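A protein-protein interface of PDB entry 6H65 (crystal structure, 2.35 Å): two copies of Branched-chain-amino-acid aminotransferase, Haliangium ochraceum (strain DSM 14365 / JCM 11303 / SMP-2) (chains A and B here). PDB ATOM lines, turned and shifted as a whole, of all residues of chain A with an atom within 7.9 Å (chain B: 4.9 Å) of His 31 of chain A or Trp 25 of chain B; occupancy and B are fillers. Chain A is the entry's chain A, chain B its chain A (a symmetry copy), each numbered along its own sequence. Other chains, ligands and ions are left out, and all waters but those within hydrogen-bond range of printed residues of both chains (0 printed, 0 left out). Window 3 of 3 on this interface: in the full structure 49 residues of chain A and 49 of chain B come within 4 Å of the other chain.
1 position is printed for both chains.
Of the 5 pairs that touch across the chains among the printed residues, none has its exchanged pair printed and touching as well.
Of the 14 printed residues of chain A, 3 touch a printed residue of chain B.
Printed residues of chain A that touch a printed residue of chain B: Leu 30, His 31 and Val 32.
Of the 13 printed residues of chain B, 4 touch a printed residue of chain A.
Hydrophobic or aromatic side chains of chain B within 4 Å of the printed part of chain A: Trp 25.
Among the printed residues, 5 pairs touch across the chains.
Among the printed residues, no Asp or Glu carboxylate lies within 4 Å of a Lys or Arg side-chain nitrogen of the other chain.
OG of Ser 33 of chain A sits at hydrogen-bond distance from ND1 of His 31 of chain A (2.9 Å).
The backbone carbonyl oxygen (O) of Pro 24 of chain B is in hydrogen-bond range of the side-chain sulfur (SG) of Cys 28 of chain B, at 3.7 Å.
The backbone carbonyl oxygen of His 31 of chain A sits at hydrogen-bond distance from the side-chain hydroxyl of Thr 34 of chain A, 3.0 Å away.
The backbone NH (N) of Trp 25 of chain B lies within hydrogen-bond range of the backbone carbonyl oxygen (O) of Arg 14 of chain B.
NE2 of His 31 of chain A is in hydrogen-bond range of O of Trp 25 of chain B (2.9 Å).
O of Cys 28 of chain B lies within hydrogen-bond range of N of Val 32 of chain A, at 2.9 Å.
Ser 29 of chain B touches Leu 30 of chain A (CA to O, 3.3 Å).
Asp 26 of chain B touches His 31 of chain A.
CA of His 31 of chain A touches O of Cys 28 of chain B, 3.5 Å away.
His 31 of chain A touches just these residues of chain B: Trp 25, Asp 26 and Cys 28.
Of the printed residues of chain A, Trp 25 of chain B touches His 31.
Of the printed residues of chain B, Val 32 of chain A touches Cys 28 (2.9 Å).
Printed residues of chain A within 4 Å of Asp 26 of chain B: His 31 (3.97 Å).
Of the printed residues of chain B, Leu 30 of chain A touches Ser 29 (3.3 Å).
Ser 33 of chain A touches none of the printed residues of chain B.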
ATOM      1  N   SER A  29     -12.137   6.253   2.621  1.00  0.00           N
ATOM      2  CA  SER A  29     -13.355   5.825   1.958  1.00  0.00           C
ATOM      3  C   SER A  29     -13.308   6.080   0.459  1.00  0.00           C
ATOM      4  O   SER A  29     -12.719   7.069   0.042  1.00  0.00           O
ATOM      5  CB  SER A  29     -14.455   6.626   2.505  1.00  0.00           C
ATOM      6  OG  SER A  29     -14.963   5.924   3.597  1.00  0.00           O
ATOM      7  N   LEU A  30     -13.980   5.226  -0.319  1.00  0.00           N
ATOM      8  CA  LEU A  30     -14.219   5.478  -1.735  1.00  0.00           C
ATOM      9  C   LEU A  30     -15.724   5.442  -2.011  1.00  0.00           C
ATOM     10  O   LEU A  30     -16.474   4.663  -1.449  1.00  0.00           O
ATOM     11  CB  LEU A  30     -13.478   4.457  -2.593  1.00  0.00           C
ATOM     12  CG  LEU A  30     -11.963   4.410  -2.418  1.00  0.00           C
ATOM     13  CD1 LEU A  30     -11.374   3.115  -2.991  1.00  0.00           C
ATOM     14  CD2 LEU A  30     -11.243   5.657  -2.946  1.00  0.00           C
ATOM     15  N   HIS A  31     -16.194   6.316  -2.885  1.00  0.00           N
ATOM     16  CA  HIS A  31     -17.574   6.272  -3.334  1.00  0.00           C
ATOM     17  C   HIS A  31     -17.835   4.949  -4.063  1.00  0.00           C
ATOM     18  O   HIS A  31     -16.942   4.375  -4.706  1.00  0.00           O
ATOM     19  CB  HIS A  31     -17.825   7.498  -4.192  1.00  0.00           C
ATOM     20  CG  HIS A  31     -19.261   7.744  -4.390  1.00  0.00           C
ATOM     21  ND1 HIS A  31     -19.983   7.054  -5.323  1.00  0.00           N
ATOM     22  CD2 HIS A  31     -20.101   8.600  -3.780  1.00  0.00           C
ATOM     23  CE1 HIS A  31     -21.229   7.491  -5.293  1.00  0.00           C
ATOM     24  NE2 HIS A  31     -21.320   8.459  -4.378  1.00  0.00           N
ATOM     25  N   VAL A  32     -19.072   4.456  -3.949  1.00  0.00           N
ATOM     26  CA  VAL A  32     -19.372   3.118  -4.438  1.00  0.00           C
ATOM     27  C   VAL A  32     -19.280   3.127  -5.956  1.00  0.00           C
ATOM     28  O   VAL A  32     -19.046   2.087  -6.565  1.00  0.00           O
ATOM     29  CB  VAL A  32     -20.764   2.620  -3.988  1.00  0.00           C
ATOM     30  CG1 VAL A  32     -20.776   2.227  -2.506  1.00  0.00           C
ATOM     31  CG2 VAL A  32     -21.895   3.594  -4.344  1.00  0.00           C
ATOM     32  N   SER A  33     -19.459   4.303  -6.560  1.00  0.00           N
ATOM     33  CA  SER A  33     -19.397   4.383  -8.009  1.00  0.00           C
ATOM     34  C   SER A  33     -17.959   4.499  -8.549  1.00  0.00           C
ATOM     35  O   SER A  33     -17.803   4.554  -9.755  1.00  0.00           O
ATOM     36  CB  SER A  33     -20.246   5.499  -8.512  1.00  0.00           C
ATOM     37  OG  SER A  33     -19.631   6.728  -8.203  1.00  0.00           O
ATOM     38  N   THR A  34     -16.914   4.532  -7.709  1.00  0.00           N
ATOM     39  CA  THR A  34     -15.573   4.581  -8.262  1.00  0.00           C
ATOM     40  C   THR A  34     -15.201   3.220  -8.846  1.00  0.00           C
ATOM     41  O   THR A  34     -15.700   2.192  -8.374  1.00  0.00           O
ATOM     42  CB  THR A  34     -14.492   4.957  -7.235  1.00  0.00           C
ATOM     43  OG1 THR A  34     -14.374   3.918  -6.272  1.00  0.00           O
ATOM     44  CG2 THR A  34     -14.687   6.330  -6.622  1.00  0.00           C
ATOM     45  N   GLN A  35     -14.289   3.206  -9.833  1.00  0.00           N
ATOM     46  CA  GLN A  35     -13.911   1.947 -10.417  1.00  0.00           C
ATOM     47  C   GLN A  35     -13.229   1.109  -9.340  1.00  0.00           C
ATOM     48  O   GLN A  35     -13.323  -0.127  -9.324  1.00  0.00           O
ATOM     49  CB  GLN A  35     -13.062   2.118 -11.668  1.00  0.00           C
ATOM     50  CG  GLN A  35     -13.760   2.862 -12.788  1.00  0.00           C
ATOM     51  CD  GLN A  35     -12.981   2.949 -14.085  1.00  0.00           C
ATOM     52  OE1 GLN A  35     -11.843   2.566 -14.192  1.00  0.00           O
ATOM     53  NE2 GLN A  35     -13.592   3.499 -15.105  1.00  0.00           N
ATOM     54  N   ALA A  36     -12.555   1.793  -8.407  1.00  0.00           N
ATOM     55  CA  ALA A  36     -11.827   1.061  -7.383  1.00  0.00           C
ATOM     56  C   ALA A  36     -12.806   0.267  -6.519  1.00  0.00           C
ATOM     57  O   ALA A  36     -12.677  -0.947  -6.401  1.00  0.00           O
ATOM     58  CB  ALA A  36     -10.977   2.010  -6.577  1.00  0.00           C
ATOM     59  N   ALA A  37     -13.797   0.958  -5.951  1.00  0.00           N
ATOM     60  CA  ALA A  37     -14.792   0.346  -5.076  1.00  0.00           C
ATOM     61  C   ALA A  37     -15.572  -0.747  -5.807  1.00  0.00           C
ATOM     62  O   ALA A  37     -15.770  -1.825  -5.281  1.00  0.00           O
ATOM     63  CB  ALA A  37     -15.726   1.402  -4.519  1.00  0.00           C
ATOM     64  N   PHE A  38     -15.987  -0.471  -7.041  1.00  0.00           N
ATOM     65  CA  PHE A  38     -16.955  -1.311  -7.730  1.00  0.00           C
ATOM     66  C   PHE A  38     -16.276  -2.543  -8.334  1.00  0.00           C
ATOM     67  O   PHE A  38     -16.768  -3.666  -8.171  1.00  0.00           O
ATOM     68  CB  PHE A  38     -17.707  -0.469  -8.749  1.00  0.00           C
ATOM     69  CG  PHE A  38     -18.840  -1.195  -9.396  1.00  0.00           C
ATOM     70  CD1 PHE A  38     -20.083  -1.239  -8.782  1.00  0.00           C
ATOM     71  CD2 PHE A  38     -18.649  -1.892 -10.579  1.00  0.00           C
ATOM     72  CE1 PHE A  38     -21.138  -1.936  -9.368  1.00  0.00           C
ATOM     73  CE2 PHE A  38     -19.703  -2.578 -11.172  1.00  0.00           C
ATOM     74  CZ  PHE A  38     -20.946  -2.603 -10.563  1.00  0.00           C
ATOM     75  N   TYR A 112      -5.345   3.643  -7.526  1.00  0.00           N
ATOM     76  CA  TYR A 112      -6.711   3.220  -7.814  1.00  0.00           C
ATOM     77  C   TYR A 112      -7.346   4.127  -8.867  1.00  0.00           C
ATOM     78  O   TYR A 112      -7.018   5.315  -8.965  1.00  0.00           O
ATOM     79  CB  TYR A 112      -7.519   3.174  -6.513  1.00  0.00           C
ATOM     80  CG  TYR A 112      -7.782   4.512  -5.856  1.00  0.00           C
ATOM     81  CD1 TYR A 112      -8.796   5.332  -6.280  1.00  0.00           C
ATOM     82  CD2 TYR A 112      -6.989   4.960  -4.797  1.00  0.00           C
ATOM     83  CE1 TYR A 112      -9.039   6.553  -5.664  1.00  0.00           C
ATOM     84  CE2 TYR A 112      -7.197   6.181  -4.183  1.00  0.00           C
ATOM     85  CZ  TYR A 112      -8.235   6.978  -4.608  1.00  0.00           C
ATOM     86  OH  TYR A 112      -8.443   8.179  -3.976  1.00  0.00           O
ATOM     87  N   PHE A 113      -8.278   3.545  -9.640  1.00  0.00           N
ATOM     88  CA  PHE A 113      -9.102   4.328 -10.539  1.00  0.00           C
ATOM     89  C   PHE A 113     -10.268   4.937  -9.769  1.00  0.00           C
ATOM     90  O   PHE A 113     -10.904   4.258  -8.959  1.00  0.00           O
ATOM     91  CB  PHE A 113      -9.630   3.435 -11.652  1.00  0.00           C
ATOM     92  CG  PHE A 113      -8.649   3.043 -12.724  1.00  0.00           C
ATOM     93  CD1 PHE A 113      -8.132   3.996 -13.605  1.00  0.00           C
ATOM     94  CD2 PHE A 113      -8.292   1.712 -12.893  1.00  0.00           C
ATOM     95  CE1 PHE A 113      -7.273   3.606 -14.614  1.00  0.00           C
ATOM     96  CE2 PHE A 113      -7.448   1.326 -13.926  1.00  0.00           C
ATOM     97  CZ  PHE A 113      -6.900   2.275 -14.744  1.00  0.00           C
ATOM     98  N   GLY A 114     -10.558   6.220 -10.044  1.00  0.00           N
ATOM     99  CA  GLY A 114     -11.665   6.912  -9.395  1.00  0.00           C
ATOM    100  C   GLY A 114     -12.961   6.890 -10.197  1.00  0.00           C
ATOM    101  O   GLY A 114     -13.378   5.834 -10.653  1.00  0.00           O
ATOM    102  N   ILE A 115     -13.602   8.071 -10.286  1.00  0.00           N
ATOM    103  CA  ILE A 115     -14.889   8.321 -10.898  1.00  0.00           C
ATOM    104  C   ILE A 115     -14.688   8.183 -12.398  1.00  0.00           C
ATOM    105  O   ILE A 115     -13.630   8.545 -12.900  1.00  0.00           O
ATOM    106  CB  ILE A 115     -15.346   9.751 -10.543  1.00  0.00           C
ATOM    107  N   PRO B  12     -25.961  14.442 -11.676  1.00  0.00           N
ATOM    108  CA  PRO B  12     -25.966  13.238 -10.791  1.00  0.00           C
ATOM    109  C   PRO B  12     -27.292  13.083 -10.032  1.00  0.00           C
ATOM    110  O   PRO B  12     -27.998  14.059  -9.777  1.00  0.00           O
ATOM    111  CB  PRO B  12     -24.831  13.432  -9.759  1.00  0.00           C
ATOM    112  CG  PRO B  12     -24.833  14.951  -9.616  1.00  0.00           C
ATOM    113  CD  PRO B  12     -25.229  15.515 -10.981  1.00  0.00           C
ATOM    114  N   PRO B  13     -27.708  11.857  -9.620  1.00  0.00           N
ATOM    115  CA  PRO B  13     -28.885  11.694  -8.753  1.00  0.00           C
ATOM    116  C   PRO B  13     -28.732  12.214  -7.326  1.00  0.00           C
ATOM    117  O   PRO B  13     -27.621  12.331  -6.810  1.00  0.00           O
ATOM    118  CB  PRO B  13     -29.051  10.181  -8.631  1.00  0.00           C
ATOM    119  CG  PRO B  13     -27.658   9.607  -8.932  1.00  0.00           C
ATOM    120  CD  PRO B  13     -27.063  10.575  -9.950  1.00  0.00           C
ATOM    121  N   ARG B  14     -29.872  12.510  -6.697  1.00  0.00           N
ATOM    122  CA  ARG B  14     -29.885  13.059  -5.350  1.00  0.00           C
ATOM    123  C   ARG B  14     -29.564  12.000  -4.298  1.00  0.00           C
ATOM    124  O   ARG B  14     -28.859  12.285  -3.322  1.00  0.00           O
ATOM    125  CB  ARG B  14     -31.244  13.707  -5.073  1.00  0.00           C
ATOM    126  CG  ARG B  14     -31.193  14.875  -4.110  1.00  0.00           C
ATOM    127  CD  ARG B  14     -32.458  15.708  -4.422  1.00  0.00           C
ATOM    128  NE  ARG B  14     -32.931  15.855  -5.813  1.00  0.00           N
ATOM    129  CZ  ARG B  14     -34.075  15.344  -6.328  1.00  0.00           C
ATOM    130  NH1 ARG B  14     -34.186  15.182  -7.637  1.00  0.00           N
ATOM    131  NH2 ARG B  14     -35.066  14.932  -5.543  1.00  0.00           N
ATOM    132  N   TYR B  15     -30.093  10.772  -4.471  1.00  0.00           N
ATOM    133  CA  TYR B  15     -29.921   9.796  -3.418  1.00  0.00           C
ATOM    134  C   TYR B  15     -29.399   8.484  -3.967  1.00  0.00           C
ATOM    135  O   TYR B  15     -29.536   8.175  -5.140  1.00  0.00           O
ATOM    136  CB  TYR B  15     -31.254   9.499  -2.742  1.00  0.00           C
ATOM    137  CG  TYR B  15     -31.945  10.704  -2.143  1.00  0.00           C
ATOM    138  CD1 TYR B  15     -31.592  11.225  -0.896  1.00  0.00           C
ATOM    139  CD2 TYR B  15     -32.988  11.303  -2.832  1.00  0.00           C
ATOM    140  CE1 TYR B  15     -32.224  12.342  -0.381  1.00  0.00           C
ATOM    141  CE2 TYR B  15     -33.642  12.409  -2.315  1.00  0.00           C
ATOM    142  CZ  TYR B  15     -33.255  12.938  -1.096  1.00  0.00           C
ATOM    143  OH  TYR B  15     -33.933  14.029  -0.611  1.00  0.00           O
ATOM    144  N   GLY B  16     -28.775   7.705  -3.086  1.00  0.00           N
ATOM    145  CA  GLY B  16     -28.654   6.267  -3.284  1.00  0.00           C
ATOM    146  C   GLY B  16     -29.271   5.552  -2.082  1.00  0.00           C
ATOM    147  O   GLY B  16     -29.782   6.209  -1.182  1.00  0.00           O
ATOM    148  N   ILE B  23     -30.078   7.671   1.227  1.00  0.00           N
ATOM    149  CA  ILE B  23     -29.112   8.561   1.837  1.00  0.00           C
ATOM    150  C   ILE B  23     -28.490   9.407   0.717  1.00  0.00           C
ATOM    151  O   ILE B  23     -28.444   8.956  -0.432  1.00  0.00           O
ATOM    152  CB  ILE B  23     -28.063   7.772   2.645  1.00  0.00           C
ATOM    153  CG1 ILE B  23     -27.295   6.784   1.773  1.00  0.00           C
ATOM    154  CG2 ILE B  23     -28.661   7.097   3.860  1.00  0.00           C
ATOM    155  CD1 ILE B  23     -25.883   6.553   2.258  1.00  0.00           C
ATOM    156  N   PRO B  24     -28.052  10.663   0.999  1.00  0.00           N
ATOM    157  CA  PRO B  24     -27.512  11.530  -0.051  1.00  0.00           C
ATOM    158  C   PRO B  24     -26.432  10.810  -0.847  1.00  0.00           C
ATOM    159  O   PRO B  24     -25.645  10.042  -0.279  1.00  0.00           O
ATOM    160  CB  PRO B  24     -26.978  12.749   0.708  1.00  0.00           C
ATOM    161  CG  PRO B  24     -27.777  12.773   2.011  1.00  0.00           C
ATOM    162  CD  PRO B  24     -28.069  11.319   2.320  1.00  0.00           C
ATOM    163  N   TRP B  25     -26.465  11.036  -2.170  1.00  0.00           N
ATOM    164  CA  TRP B  25     -25.578  10.397  -3.125  1.00  0.00           C
ATOM    165  C   TRP B  25     -24.121  10.527  -2.693  1.00  0.00           C
ATOM    166  O   TRP B  25     -23.372   9.566  -2.726  1.00  0.00           O
ATOM    167  CB  TRP B  25     -25.839  11.011  -4.493  1.00  0.00           C
ATOM    168  CG  TRP B  25     -24.910  10.577  -5.586  1.00  0.00           C
ATOM    169  CD1 TRP B  25     -24.055  11.366  -6.300  1.00  0.00           C
ATOM    170  CD2 TRP B  25     -24.766   9.251  -6.122  1.00  0.00           C
ATOM    171  NE1 TRP B  25     -23.358  10.608  -7.199  1.00  0.00           N
ATOM    172  CE2 TRP B  25     -23.757   9.306  -7.105  1.00  0.00           C
ATOM    173  CE3 TRP B  25     -25.361   8.018  -5.824  1.00  0.00           C
ATOM    174  CZ2 TRP B  25     -23.369   8.194  -7.844  1.00  0.00           C
ATOM    175  CZ3 TRP B  25     -24.931   6.897  -6.492  1.00  0.00           C
ATOM    176  CH2 TRP B  25     -23.976   6.992  -7.515  1.00  0.00           C
ATOM    177  N   ASP B  26     -23.758  11.730  -2.263  1.00  0.00           N
ATOM    178  CA  ASP B  26     -22.490  12.161  -1.704  1.00  0.00           C
ATOM    179  C   ASP B  26     -21.873  11.125  -0.757  1.00  0.00           C
ATOM    180  O   ASP B  26     -20.652  11.009  -0.672  1.00  0.00           O
ATOM    181  CB  ASP B  26     -22.783  13.511  -1.035  1.00  0.00           C
ATOM    182  CG  ASP B  26     -21.573  14.183  -0.421  1.00  0.00           C
ATOM    183  OD1 ASP B  26     -20.746  13.449   0.168  1.00  0.00           O
ATOM    184  OD2 ASP B  26     -21.470  15.441  -0.534  1.00  0.00           O
ATOM    185  N   GLN B  27     -22.688  10.460   0.056  1.00  0.00           N
ATOM    186  CA  GLN B  27     -22.049   9.706   1.124  1.00  0.00           C
ATOM    187  C   GLN B  27     -22.325   8.210   0.969  1.00  0.00           C
ATOM    188  O   GLN B  27     -22.362   7.480   1.949  1.00  0.00           O
ATOM    189  CB  GLN B  27     -22.386  10.230   2.521  1.00  0.00           C
ATOM    190  CG  GLN B  27     -22.709  11.714   2.572  1.00  0.00           C
ATOM    191  CD  GLN B  27     -23.594  12.065   3.746  1.00  0.00           C
ATOM    192  OE1 GLN B  27     -24.735  11.604   3.894  1.00  0.00           O
ATOM    193  NE2 GLN B  27     -23.067  12.925   4.603  1.00  0.00           N
ATOM    194  N   CYS B  28     -22.510   7.776  -0.281  1.00  0.00           N
ATOM    195  CA  CYS B  28     -22.601   6.370  -0.625  1.00  0.00           C
ATOM    196  C   CYS B  28     -21.198   5.774  -0.816  1.00  0.00           C
ATOM    197  O   CYS B  28     -20.704   5.668  -1.927  1.00  0.00           O
ATOM    198  CB  CYS B  28     -23.548   6.181  -1.805  1.00  0.00           C
ATOM    199  SG  CYS B  28     -25.293   6.530  -1.388  1.00  0.00           S
ATOM    200  N   SER B  29     -20.614   5.324   0.296  1.00  0.00           N
ATOM    201  CA  SER B  29     -19.188   5.105   0.463  1.00  0.00           C
ATOM    202  C   SER B  29     -18.891   3.773   1.136  1.00  0.00           C
ATOM    203  O   SER B  29     -19.662   3.353   1.989  1.00  0.00           O
ATOM    204  CB  SER B  29     -18.683   6.164   1.343  1.00  0.00           C
ATOM    205  OG  SER B  29     -18.289   7.219   0.522  1.00  0.00           O
ATOM    206  N   THR B 133     -28.234   1.710  -6.483  1.00  0.00           N
ATOM    207  CA  THR B 133     -27.838   2.937  -7.145  1.00  0.00           C
ATOM    208  C   THR B 133     -28.707   3.020  -8.384  1.00  0.00           C
ATOM    209  O   THR B 133     -28.960   2.006  -9.019  1.00  0.00           O
ATOM    210  CB  THR B 133     -26.350   2.797  -7.510  1.00  0.00           C
ATOM    211  OG1 THR B 133     -25.711   3.535  -6.469  1.00  0.00           O
ATOM    212  CG2 THR B 133     -25.953   3.228  -8.913  1.00  0.00           C
